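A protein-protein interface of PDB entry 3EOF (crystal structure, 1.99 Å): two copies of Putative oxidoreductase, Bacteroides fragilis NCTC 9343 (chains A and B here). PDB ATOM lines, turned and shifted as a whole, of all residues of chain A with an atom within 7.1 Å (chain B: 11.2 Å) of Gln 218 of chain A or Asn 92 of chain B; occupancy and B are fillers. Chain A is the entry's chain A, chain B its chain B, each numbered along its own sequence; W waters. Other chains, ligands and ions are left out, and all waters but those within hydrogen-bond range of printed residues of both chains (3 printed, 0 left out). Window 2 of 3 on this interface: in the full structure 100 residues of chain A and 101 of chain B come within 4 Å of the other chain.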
ATOM      1  N   ILE A 208       5.648  23.658   6.067  1.00  0.00           N
ATOM      2  CA  ILE A 208       4.840  23.058   4.983  1.00  0.00           C
ATOM      3  C   ILE A 208       4.482  24.088   3.919  1.00  0.00           C
ATOM      4  O   ILE A 208       4.582  23.847   2.705  1.00  0.00           O
ATOM      5  CB  ILE A 208       3.501  22.483   5.559  1.00  0.00           C
ATOM      6  CG1 ILE A 208       3.747  21.309   6.508  1.00  0.00           C
ATOM      7  CG2 ILE A 208       2.560  22.073   4.448  1.00  0.00           C
ATOM      8  CD1 ILE A 208       2.518  20.972   7.440  1.00  0.00           C
ATOM      9  N   ASN A 211       7.269  25.398   1.751  1.00  0.00           N
ATOM     10  CA  ASN A 211       7.810  24.342   0.909  1.00  0.00           C
ATOM     11  C   ASN A 211       6.829  23.826  -0.144  1.00  0.00           C
ATOM     12  O   ASN A 211       7.145  22.905  -0.870  1.00  0.00           O
ATOM     13  CB  ASN A 211       8.382  23.228   1.780  1.00  0.00           C
ATOM     14  CG  ASN A 211       9.773  23.541   2.259  1.00  0.00           C
ATOM     15  OD1 ASN A 211      10.706  23.562   1.454  1.00  0.00           O
ATOM     16  ND2 ASN A 211       9.937  23.759   3.566  1.00  0.00           N
ATOM     17  N   GLN A 212       5.666  24.469  -0.244  1.00  0.00           N
ATOM     18  CA  GLN A 212       4.629  24.149  -1.218  1.00  0.00           C
ATOM     19  C   GLN A 212       4.051  22.750  -1.055  1.00  0.00           C
ATOM     20  O   GLN A 212       3.620  22.141  -2.029  1.00  0.00           O
ATOM     21  CB  GLN A 212       5.164  24.284  -2.656  1.00  0.00           C
ATOM     22  CG  GLN A 212       5.930  25.562  -2.993  1.00  0.00           C
ATOM     23  CD  GLN A 212       5.069  26.792  -2.906  1.00  0.00           C
ATOM     24  OE1 GLN A 212       4.613  27.178  -1.823  1.00  0.00           O
ATOM     25  NE2 GLN A 212       4.857  27.440  -4.052  1.00  0.00           N
ATOM     26  N   LYS A 213       3.993  22.263   0.176  1.00  0.00           N
ATOM     27  CA  LYS A 213       3.521  20.901   0.448  1.00  0.00           C
ATOM     28  C   LYS A 213       2.208  20.971   1.174  1.00  0.00           C
ATOM     29  O   LYS A 213       1.780  22.049   1.565  1.00  0.00           O
ATOM     30  CB  LYS A 213       4.561  20.123   1.281  1.00  0.00           C
ATOM     31  CG  LYS A 213       5.913  19.946   0.580  1.00  0.00           C
ATOM     32  CD  LYS A 213       5.760  19.237  -0.782  1.00  0.00           C
ATOM     33  CE  LYS A 213       7.058  19.235  -1.586  1.00  0.00           C
ATOM     34  NZ  LYS A 213       6.807  18.509  -2.856  1.00  0.00           N
ATOM     35  N   GLU A 214       1.565  19.824   1.337  1.00  0.00           N
ATOM     36  CA  GLU A 214       0.285  19.751   2.020  1.00  0.00           C
ATOM     37  C   GLU A 214       0.474  19.205   3.414  1.00  0.00           C
ATOM     38  O   GLU A 214      -0.216  19.609   4.342  1.00  0.00           O
ATOM     39  CB  GLU A 214      -0.697  18.933   1.162  1.00  0.00           C
ATOM     40  CG  GLU A 214      -1.031  19.726  -0.139  1.00  0.00           C
ATOM     41  CD  GLU A 214      -1.876  18.999  -1.202  1.00  0.00           C
ATOM     42  OE1 GLU A 214      -2.155  17.778  -1.079  1.00  0.00           O
ATOM     43  OE2 GLU A 214      -2.235  19.675  -2.204  1.00  0.00           O
ATOM     44  N   THR A 215       1.453  18.325   3.590  1.00  0.00           N
ATOM     45  CA  THR A 215       1.717  17.718   4.899  1.00  0.00           C
ATOM     46  C   THR A 215       3.188  17.834   5.294  1.00  0.00           C
ATOM     47  O   THR A 215       4.090  18.010   4.456  1.00  0.00           O
ATOM     48  CB  THR A 215       1.311  16.242   4.895  1.00  0.00           C
ATOM     49  OG1 THR A 215       2.251  15.507   4.139  1.00  0.00           O
ATOM     50  CG2 THR A 215      -0.069  16.043   4.274  1.00  0.00           C
ATOM     51  N   LEU A 216       3.427  17.726   6.589  1.00  0.00           N
ATOM     52  CA  LEU A 216       4.761  17.843   7.121  1.00  0.00           C
ATOM     53  C   LEU A 216       5.746  16.778   6.552  1.00  0.00           C
ATOM     54  O   LEU A 216       6.807  17.136   6.060  1.00  0.00           O
ATOM     55  CB  LEU A 216       4.710  17.874   8.661  1.00  0.00           C
ATOM     56  CG  LEU A 216       6.044  18.076   9.365  1.00  0.00           C
ATOM     57  CD1 LEU A 216       6.651  19.404   8.883  1.00  0.00           C
ATOM     58  CD2 LEU A 216       5.843  18.043  10.865  1.00  0.00           C
ATOM     59  N   PRO A 217       5.387  15.479   6.588  1.00  0.00           N
ATOM     60  CA  PRO A 217       6.255  14.470   6.006  1.00  0.00           C
ATOM     61  C   PRO A 217       6.645  14.706   4.561  1.00  0.00           C
ATOM     62  O   PRO A 217       7.711  14.295   4.162  1.00  0.00           O
ATOM     63  CB  PRO A 217       5.413  13.191   6.116  1.00  0.00           C
ATOM     64  CG  PRO A 217       4.599  13.406   7.281  1.00  0.00           C
ATOM     65  CD  PRO A 217       4.200  14.848   7.190  1.00  0.00           C
ATOM     66  N   GLN A 218       5.799  15.348   3.770  1.00  0.00           N
ATOM     67  CA  GLN A 218       6.152  15.634   2.387  1.00  0.00           C
ATOM     68  C   GLN A 218       7.359  16.559   2.309  1.00  0.00           C
ATOM     69  O   GLN A 218       8.132  16.466   1.362  1.00  0.00           O
ATOM     70  CB  GLN A 218       4.995  16.252   1.631  1.00  0.00           C
ATOM     71  CG  GLN A 218       3.876  15.271   1.340  1.00  0.00           C
ATOM     72  CD  GLN A 218       2.598  15.934   0.927  1.00  0.00           C
ATOM     73  OE1 GLN A 218       2.473  17.152   0.970  1.00  0.00           O
ATOM     74  NE2 GLN A 218       1.636  15.141   0.513  1.00  0.00           N
ATOM     75  N   VAL A 219       7.531  17.444   3.295  1.00  0.00           N
ATOM     76  CA  VAL A 219       8.673  18.349   3.255  1.00  0.00           C
ATOM     77  C   VAL A 219       9.926  17.494   3.420  1.00  0.00           C
ATOM     78  O   VAL A 219      10.942  17.702   2.762  1.00  0.00           O
ATOM     79  CB  VAL A 219       8.598  19.418   4.330  1.00  0.00           C
ATOM     80  CG1 VAL A 219       9.840  20.323   4.257  1.00  0.00           C
ATOM     81  CG2 VAL A 219       7.293  20.238   4.170  1.00  0.00           C
ATOM     82  N   PHE A 220       9.854  16.520   4.307  1.00  0.00           N
ATOM     83  CA  PHE A 220      10.988  15.643   4.504  1.00  0.00           C
ATOM     84  C   PHE A 220      11.310  14.713   3.350  1.00  0.00           C
ATOM     85  O   PHE A 220      12.472  14.557   2.992  1.00  0.00           O
ATOM     86  CB  PHE A 220      10.789  14.847   5.776  1.00  0.00           C
ATOM     87  CG  PHE A 220      10.893  15.683   6.997  1.00  0.00           C
ATOM     88  CD1 PHE A 220      12.116  15.917   7.577  1.00  0.00           C
ATOM     89  CD2 PHE A 220       9.783  16.255   7.555  1.00  0.00           C
ATOM     90  CE1 PHE A 220      12.223  16.712   8.660  1.00  0.00           C
ATOM     91  CE2 PHE A 220       9.897  17.035   8.676  1.00  0.00           C
ATOM     92  CZ  PHE A 220      11.109  17.267   9.219  1.00  0.00           C
ATOM     93  N   THR A 221      10.279  14.091   2.780  1.00  0.00           N
ATOM     94  CA  THR A 221      10.447  13.116   1.717  1.00  0.00           C
ATOM     95  C   THR A 221      10.706  13.775   0.373  1.00  0.00           C
ATOM     96  O   THR A 221      11.438  13.237  -0.436  1.00  0.00           O
ATOM     97  CB  THR A 221       9.178  12.228   1.554  1.00  0.00           C
ATOM     98  OG1 THR A 221       8.071  13.025   1.102  1.00  0.00           O
ATOM     99  CG2 THR A 221       8.792  11.567   2.871  1.00  0.00           C
ATOM    100  N   ASP A 222      10.096  14.927   0.134  1.00  0.00           N
ATOM    101  CA  ASP A 222      10.243  15.602  -1.158  1.00  0.00           C
ATOM    102  C   ASP A 222      11.363  16.634  -1.271  1.00  0.00           C
ATOM    103  O   ASP A 222      11.853  16.918  -2.380  1.00  0.00           O
ATOM    104  CB  ASP A 222       8.918  16.262  -1.547  1.00  0.00           C
ATOM    105  CG  ASP A 222       7.755  15.259  -1.671  1.00  0.00           C
ATOM    106  OD1 ASP A 222       7.933  14.029  -1.430  1.00  0.00           O
ATOM    107  OD2 ASP A 222       6.641  15.720  -1.996  1.00  0.00           O
ATOM    108  N   VAL A 223      11.748  17.218  -0.146  1.00  0.00           N
ATOM    109  CA  VAL A 223      12.712  18.319  -0.142  1.00  0.00           C
ATOM    110  C   VAL A 223      13.971  18.050   0.686  1.00  0.00           C
ATOM    111  O   VAL A 223      15.075  18.105   0.170  1.00  0.00           O
ATOM    112  CB  VAL A 223      12.016  19.629   0.395  1.00  0.00           C
ATOM    113  CG1 VAL A 223      13.011  20.763   0.481  1.00  0.00           C
ATOM    114  CG2 VAL A 223      10.794  20.002  -0.467  1.00  0.00           C
ATOM    115  N   ARG A 224      13.804  17.745   1.963  1.00  0.00           N
ATOM    116  CA  ARG A 224      14.942  17.613   2.874  1.00  0.00           C
ATOM    117  C   ARG A 224      15.764  16.336   2.706  1.00  0.00           C
ATOM    118  O   ARG A 224      16.980  16.388   2.579  1.00  0.00           O
ATOM    119  CB  ARG A 224      14.492  17.688   4.351  1.00  0.00           C
ATOM    120  CG  ARG A 224      13.934  19.006   4.839  1.00  0.00           C
ATOM    121  CD  ARG A 224      14.976  20.094   5.139  1.00  0.00           C
ATOM    122  NE  ARG A 224      15.971  19.724   6.169  1.00  0.00           N
ATOM    123  CZ  ARG A 224      15.753  19.643   7.490  1.00  0.00           C
ATOM    124  NH1 ARG A 224      14.551  19.848   8.012  1.00  0.00           N
ATOM    125  NH2 ARG A 224      16.744  19.320   8.307  1.00  0.00           N
ATOM    126  N   THR A 226      15.406  13.292   0.516  1.00  0.00           N
ATOM    127  CA  THR A 226      14.759  12.641  -0.604  1.00  0.00           C
ATOM    128  C   THR A 226      15.314  11.258  -0.899  1.00  0.00           C
ATOM    129  O   THR A 226      16.450  10.920  -0.535  1.00  0.00           O
ATOM    130  CB  THR A 226      14.846  13.504  -1.892  1.00  0.00           C
ATOM    131  OG1 THR A 226      16.195  13.576  -2.325  1.00  0.00           O
ATOM    132  CG2 THR A 226      14.319  14.922  -1.659  1.00  0.00           C
ATOM    133  N   MET B  41      13.592  14.464  13.883  1.00  0.00           N
ATOM    134  CA  MET B  41      12.789  13.302  13.496  1.00  0.00           C
ATOM    135  C   MET B  41      12.692  12.201  14.478  1.00  0.00           C
ATOM    136  O   MET B  41      11.750  11.446  14.408  1.00  0.00           O
ATOM    137  CB  MET B  41      13.278  12.731  12.151  1.00  0.00           C
ATOM    138  CG  MET B  41      13.200  13.710  11.011  1.00  0.00           C
ATOM    139  SD  MET B  41      14.199  13.134   9.464  1.00  0.00           S
ATOM    140  CE  MET B  41      12.931  12.156   8.594  1.00  0.00           C
ATOM    141  N   PHE B  84       8.629   7.006  11.319  1.00  0.00           N
ATOM    142  CA  PHE B  84       8.540   8.094  10.399  1.00  0.00           C
ATOM    143  C   PHE B  84       7.935   7.681   9.075  1.00  0.00           C
ATOM    144  O   PHE B  84       7.197   8.434   8.493  1.00  0.00           O
ATOM    145  CB  PHE B  84       9.888   8.750  10.142  1.00  0.00           C
ATOM    146  CG  PHE B  84       9.782   9.978   9.324  1.00  0.00           C
ATOM    147  CD1 PHE B  84       9.317  11.146   9.891  1.00  0.00           C
ATOM    148  CD2 PHE B  84      10.088   9.967   7.960  1.00  0.00           C
ATOM    149  CE1 PHE B  84       9.198  12.299   9.139  1.00  0.00           C
ATOM    150  CE2 PHE B  84       9.967  11.127   7.189  1.00  0.00           C
ATOM    151  CZ  PHE B  84       9.501  12.290   7.773  1.00  0.00           C
ATOM    152  N   CYS B  85       8.260   6.498   8.579  1.00  0.00           N
ATOM    153  CA  CYS B  85       7.662   6.017   7.314  1.00  0.00           C
ATOM    154  C   CYS B  85       6.167   5.789   7.445  1.00  0.00           C
ATOM    155  O   CYS B  85       5.442   6.077   6.510  1.00  0.00           O
ATOM    156  CB  CYS B  85       8.356   4.759   6.846  1.00  0.00           C
ATOM    157  SG  CYS B  85      10.007   5.196   6.228  1.00  0.00           S
ATOM    158  N   LYS B  86       5.722   5.286   8.606  1.00  0.00           N
ATOM    159  CA  LYS B  86       4.285   5.094   8.854  1.00  0.00           C
ATOM    160  C   LYS B  86       3.616   6.466   8.818  1.00  0.00           C
ATOM    161  O   LYS B  86       2.601   6.667   8.151  1.00  0.00           O
ATOM    162  CB  LYS B  86       4.006   4.300  10.173  1.00  0.00           C
ATOM    163  CG  LYS B  86       4.621   2.854  10.120  1.00  0.00           C
ATOM    164  CD  LYS B  86       4.033   1.714  11.078  1.00  0.00           C
ATOM    165  CE  LYS B  86       2.971   0.798  10.425  1.00  0.00           C
ATOM    166  NZ  LYS B  86       3.427   0.046   9.196  1.00  0.00           N
ATOM    167  N   TYR B  87       4.230   7.431   9.488  1.00  0.00           N
ATOM    168  CA  TYR B  87       3.762   8.837   9.470  1.00  0.00           C
ATOM    169  C   TYR B  87       3.631   9.335   8.052  1.00  0.00           C
ATOM    170  O   TYR B  87       2.616   9.920   7.690  1.00  0.00           O
ATOM    171  CB  TYR B  87       4.711   9.701  10.278  1.00  0.00           C
ATOM    172  CG  TYR B  87       4.378  11.169  10.363  1.00  0.00           C
ATOM    173  CD1 TYR B  87       3.067  11.604  10.499  1.00  0.00           C
ATOM    174  CD2 TYR B  87       5.393  12.122  10.440  1.00  0.00           C
ATOM    175  CE1 TYR B  87       2.769  12.935  10.629  1.00  0.00           C
ATOM    176  CE2 TYR B  87       5.096  13.475  10.578  1.00  0.00           C
ATOM    177  CZ  TYR B  87       3.787  13.878  10.659  1.00  0.00           C
ATOM    178  OH  TYR B  87       3.460  15.221  10.773  1.00  0.00           O
ATOM    179  N   CYS B  88       4.662   9.091   7.236  1.00  0.00           N
ATOM    180  CA  CYS B  88       4.623   9.466   5.809  1.00  0.00           C
ATOM    181  C   CYS B  88       3.439   8.837   5.079  1.00  0.00           C
ATOM    182  O   CYS B  88       2.789   9.464   4.239  1.00  0.00           O
ATOM    183  CB  CYS B  88       5.919   9.055   5.086  1.00  0.00           C
ATOM    184  SG  CYS B  88       7.404   9.934   5.604  1.00  0.00           S
ATOM    185  N   GLN B  89       3.190   7.580   5.397  1.00  0.00           N
ATOM    186  CA  GLN B  89       2.138   6.803   4.770  1.00  0.00           C
ATOM    187  C   GLN B  89       0.763   7.300   5.131  1.00  0.00           C
ATOM    188  O   GLN B  89      -0.178   7.127   4.353  1.00  0.00           O
ATOM    189  CB  GLN B  89       2.295   5.315   5.134  1.00  0.00           C
ATOM    190  CG  GLN B  89       3.540   4.633   4.493  1.00  0.00           C
ATOM    191  CD  GLN B  89       3.931   3.283   5.153  1.00  0.00           C
ATOM    192  OE1 GLN B  89       3.170   2.696   5.943  1.00  0.00           O
ATOM    193  NE2 GLN B  89       5.135   2.806   4.833  1.00  0.00           N
ATOM    194  N   GLU B  90       0.658   7.912   6.314  1.00  0.00           N
ATOM    195  CA  GLU B  90      -0.576   8.500   6.773  1.00  0.00           C
ATOM    196  C   GLU B  90      -0.684   9.958   6.350  1.00  0.00           C
ATOM    197  O   GLU B  90      -1.680  10.587   6.649  1.00  0.00           O
ATOM    198  CB  GLU B  90      -0.735   8.349   8.293  1.00  0.00           C
ATOM    199  CG  GLU B  90      -0.855   6.915   8.733  1.00  0.00           C
ATOM    200  CD  GLU B  90      -2.002   6.160   8.039  1.00  0.00           C
ATOM    201  OE1 GLU B  90      -3.069   6.777   7.776  1.00  0.00           O
ATOM    202  OE2 GLU B  90      -1.806   4.963   7.750  1.00  0.00           O
ATOM    203  N   ARG B  91       0.308  10.478   5.611  1.00  0.00           N
ATOM    204  CA  ARG B  91       0.285  11.854   5.176  1.00  0.00           C
ATOM    205  C   ARG B  91       0.595  12.035   3.695  1.00  0.00           C
ATOM    206  O   ARG B  91       1.167  13.053   3.278  1.00  0.00           O
ATOM    207  CB  ARG B  91       1.287  12.643   5.990  1.00  0.00           C
ATOM    208  CG  ARG B  91       0.924  12.802   7.470  1.00  0.00           C
ATOM    209  CD  ARG B  91      -0.379  13.551   7.667  1.00  0.00           C
ATOM    210  NE  ARG B  91      -0.672  13.732   9.094  1.00  0.00           N
ATOM    211  CZ  ARG B  91      -1.367  12.889   9.864  1.00  0.00           C
ATOM    212  NH1 ARG B  91      -1.879  11.787   9.382  1.00  0.00           N
ATOM    213  NH2 ARG B  91      -1.558  13.189  11.154  1.00  0.00           N
ATOM    214  N   ASN B  92       0.246  11.052   2.900  1.00  0.00           N
ATOM    215  CA  ASN B  92       0.445  11.153   1.440  1.00  0.00           C
ATOM    216  C   ASN B  92       1.871  11.567   1.019  1.00  0.00           C
ATOM    217  O   ASN B  92       2.081  12.386   0.105  1.00  0.00           O
ATOM    218  CB  ASN B  92      -0.586  12.113   0.885  1.00  0.00           C
ATOM    219  CG  ASN B  92      -0.710  12.021  -0.591  1.00  0.00           C
ATOM    220  OD1 ASN B  92      -0.534  10.966  -1.167  1.00  0.00           O
ATOM    221  ND2 ASN B  92      -1.032  13.125  -1.211  1.00  0.00           N
ATOM    222  N   ALA B  93       2.847  10.964   1.691  1.00  0.00           N
ATOM    223  CA  ALA B  93       4.271  11.181   1.439  1.00  0.00           C
ATOM    224  C   ALA B  93       4.948   9.847   1.100  1.00  0.00           C
ATOM    225  O   ALA B  93       4.712   8.815   1.735  1.00  0.00           O
ATOM    226  CB  ALA B  93       4.936  11.840   2.659  1.00  0.00           C
ATOM    227  N   VAL B  94       5.776   9.862   0.062  1.00  0.00           N
ATOM    228  CA  VAL B  94       6.518   8.674  -0.349  1.00  0.00           C
ATOM    229  C   VAL B  94       7.918   8.660   0.302  1.00  0.00           C
ATOM    230  O   VAL B  94       8.785   9.440  -0.087  1.00  0.00           O
ATOM    231  CB  VAL B  94       6.673   8.637  -1.900  1.00  0.00           C
ATOM    232  CG1 VAL B  94       7.511   7.452  -2.297  1.00  0.00           C
ATOM    233  CG2 VAL B  94       5.297   8.636  -2.578  1.00  0.00           C
ATOM    234  N   PRO B  95       8.140   7.792   1.303  1.00  0.00           N
ATOM    235  CA  PRO B  95       9.430   7.811   1.954  1.00  0.00           C
ATOM    236  C   PRO B  95      10.463   7.040   1.151  1.00  0.00           C
ATOM    237  O   PRO B  95      10.128   6.069   0.456  1.00  0.00           O
ATOM    238  CB  PRO B  95       9.144   7.130   3.285  1.00  0.00           C
ATOM    239  CG  PRO B  95       7.999   6.275   3.064  1.00  0.00           C
ATOM    240  CD  PRO B  95       7.245   6.793   1.903  1.00  0.00           C
ATOM    241  N   GLY B  96      11.694   7.503   1.202  1.00  0.00           N
ATOM    242  CA  GLY B  96      12.790   6.830   0.533  1.00  0.00           C
ATOM    243  C   GLY B  96      13.907   6.608   1.522  1.00  0.00           C
ATOM    244  O   GLY B  96      15.021   7.049   1.302  1.00  0.00           O
ATOM    245  N   TYR B  97      13.620   5.862   2.581  1.00  0.00           N
ATOM    246  CA  TYR B  97      14.573   5.662   3.680  1.00  0.00           C
ATOM    247  C   TYR B  97      15.050   4.216   3.900  1.00  0.00           C
ATOM    248  O   TYR B  97      15.658   3.915   4.928  1.00  0.00           O
ATOM    249  CB  TYR B  97      13.994   6.221   4.983  1.00  0.00           C
ATOM    250  CG  TYR B  97      13.537   7.651   4.833  1.00  0.00           C
ATOM    251  CD1 TYR B  97      14.453   8.648   4.632  1.00  0.00           C
ATOM    252  CD2 TYR B  97      12.180   8.000   4.886  1.00  0.00           C
ATOM    253  CE1 TYR B  97      14.073   9.946   4.472  1.00  0.00           C
ATOM    254  CE2 TYR B  97      11.774   9.314   4.746  1.00  0.00           C
ATOM    255  CZ  TYR B  97      12.740  10.305   4.521  1.00  0.00           C
ATOM    256  OH  TYR B  97      12.411  11.660   4.343  1.00  0.00           O
HETATM  257  O   HOH W   1       5.804  12.350  -1.595  1.00  0.00           O
HETATM  258  O   HOH W   2      12.374  10.374   0.938  1.00  0.00           O
HETATM  259  O   HOH W   3      -1.103  15.700  -0.172  1.00  0.00           O
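O of Arg 91 of chain B sits at hydrogen-bond distance from OG1 of Thr 215 of chain A (2.8 Å). The backbone carbonyl oxygen (O) of Arg 91 of chain B sits at hydrogen-bond distance from the side-chain amide nitrogen (NE2) of Gln 218 of chain A (3.5 Å). O of Asn 92 of chain B sits at hydrogen-bond distance from NE2 of Gln 218 of chain A, at 2.8 Å. O of Phe 220 of chain A sits at hydrogen-bond distance from OH of Tyr 97 of chain B (3.2 Å).
The backbone NH (N) of Glu 214 of chain A is in hydrogen-bond range of the side-chain amide oxygen (OE1) of Gln 218 of chain A (2.8 Å). The backbone NH (N) of Thr 215 of chain A sits at hydrogen-bond distance from the side-chain amide oxygen (OE1) of Gln 218 of chain A (3.0 Å). The side-chain hydroxyl of Thr 221 of chain A sits close to the backbone carbonyl oxygen of Pro 217 of chain A (3.3 Å). The side-chain hydroxyl (OG1) of Thr 221 of chain A is in hydrogen-bond range of the side-chain carboxylate (OD1) of Asp 222 of chain A, 2.7 Å away. SG of Cys 88 of chain B sits close to O of Phe 84 of chain B. The backbone carbonyl oxygen (O) of Cys 88 of chain B sits at hydrogen-bond distance from the backbone NH (N) of Ala 93 of chain B, 3.0 Å away.
Tyr 87 of chain B touches Leu 216 of chain A. CE2 of Tyr 87 of chain B touches CG of Pro 217 of chain A, at 3.3 Å. Pro 217 of chain A touches Arg 91 of chain B (CG to CB, 3.6 Å). Ala 93 of chain B touches Pro 217 of chain A (CB to CB, 3.7 Å). Gln 218 of chain A touches Ala 93 of chain B (N to CB, 3.8 Å). CG of Met 41 of chain B touches CE1 of Phe 220 of chain A, 3.9 Å away. Cys 88 of chain B touches Thr 221 of chain A. O of Val 94 of chain B touches CB of Thr 221 of chain A, at 3.3 Å. Thr 221 of chain A touches Pro 95 of chain B. OH of Tyr 97 of chain B touches CA of Thr 221 of chain A, 3.6 Å away.
No residue of chain B comes within 4 Å of Lys 213 of chain A. No residue of chain B comes within 4 Å of Glu 214 of chain A. Thr 215 of chain A touches just one residue of chain B: Arg 91 (2.8 Å). Of the printed residues of chain B, Gln 218 of chain A touches Arg 91 (3.5 Å), Asn 92 (2.8 Å) and Ala 93 (3.8 Å). Of the printed residues of chain A, Met 41 of chain B touches Phe 220 (3.9 Å). Of the printed residues of chain A, Phe 84 of chain B touches Phe 220. Of the printed residues of chain A, Cys 88 of chain B touches Pro 217 and Thr 221. Of the printed residues of chain A, Asn 92 of chain B touches Gln 218. Of the printed residues of chain A, Val 94 of chain B touches Thr 221 (3.3 Å). Printed residues of chain A within 4 Å of Pro 95 of chain B: Thr 221. The nearest residue of chain B that does not touch Gln 218 of chain A is Val 94 of chain B (5.9 Å). The nearest residue of chain A that does not touch Asn 92 of chain B is Glu 214 of chain A (4.8 Å).
Of the 16 printed residues of chain A, 6 touch a printed residue of chain B. Hydrophobic or aromatic side chains of chain A within 4 Å of the printed part of chain B: Leu 216, Pro 217 and Phe 220. Along chain A the printed residues that touch a printed residue of chain B span positions 215 to 221. Hydrophobic or aromatic side chains of chain B within 4 Å of the printed part of chain A: Met 41, Phe 84, Tyr 87, Ala 93 and Tyr 97. Among the printed residues, 17 pairs touch across the chains.
No position is printed for both chains. Of the 17 pairs that touch across the chains among the printed residues, none has its exchanged pair printed and touching as well.
Water W3 lies within hydrogen-bond range of OE1 of Glu 214 of chain A, ND2 of Asn 92 of chain B and NE2 of Gln 218 of chain A. Water W1 lies within hydrogen-bond range of OD1 of Asp 222 of chain A (2.7 Å) and N of Val 94 of chain B (3.0 Å). Water W2 lies within hydrogen-bond range of the backbone NH (N) of Gly 96 of chain B (3.0 Å) and the backbone carbonyl oxygen (O) of Thr 221 of chain A (3.3 Å).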
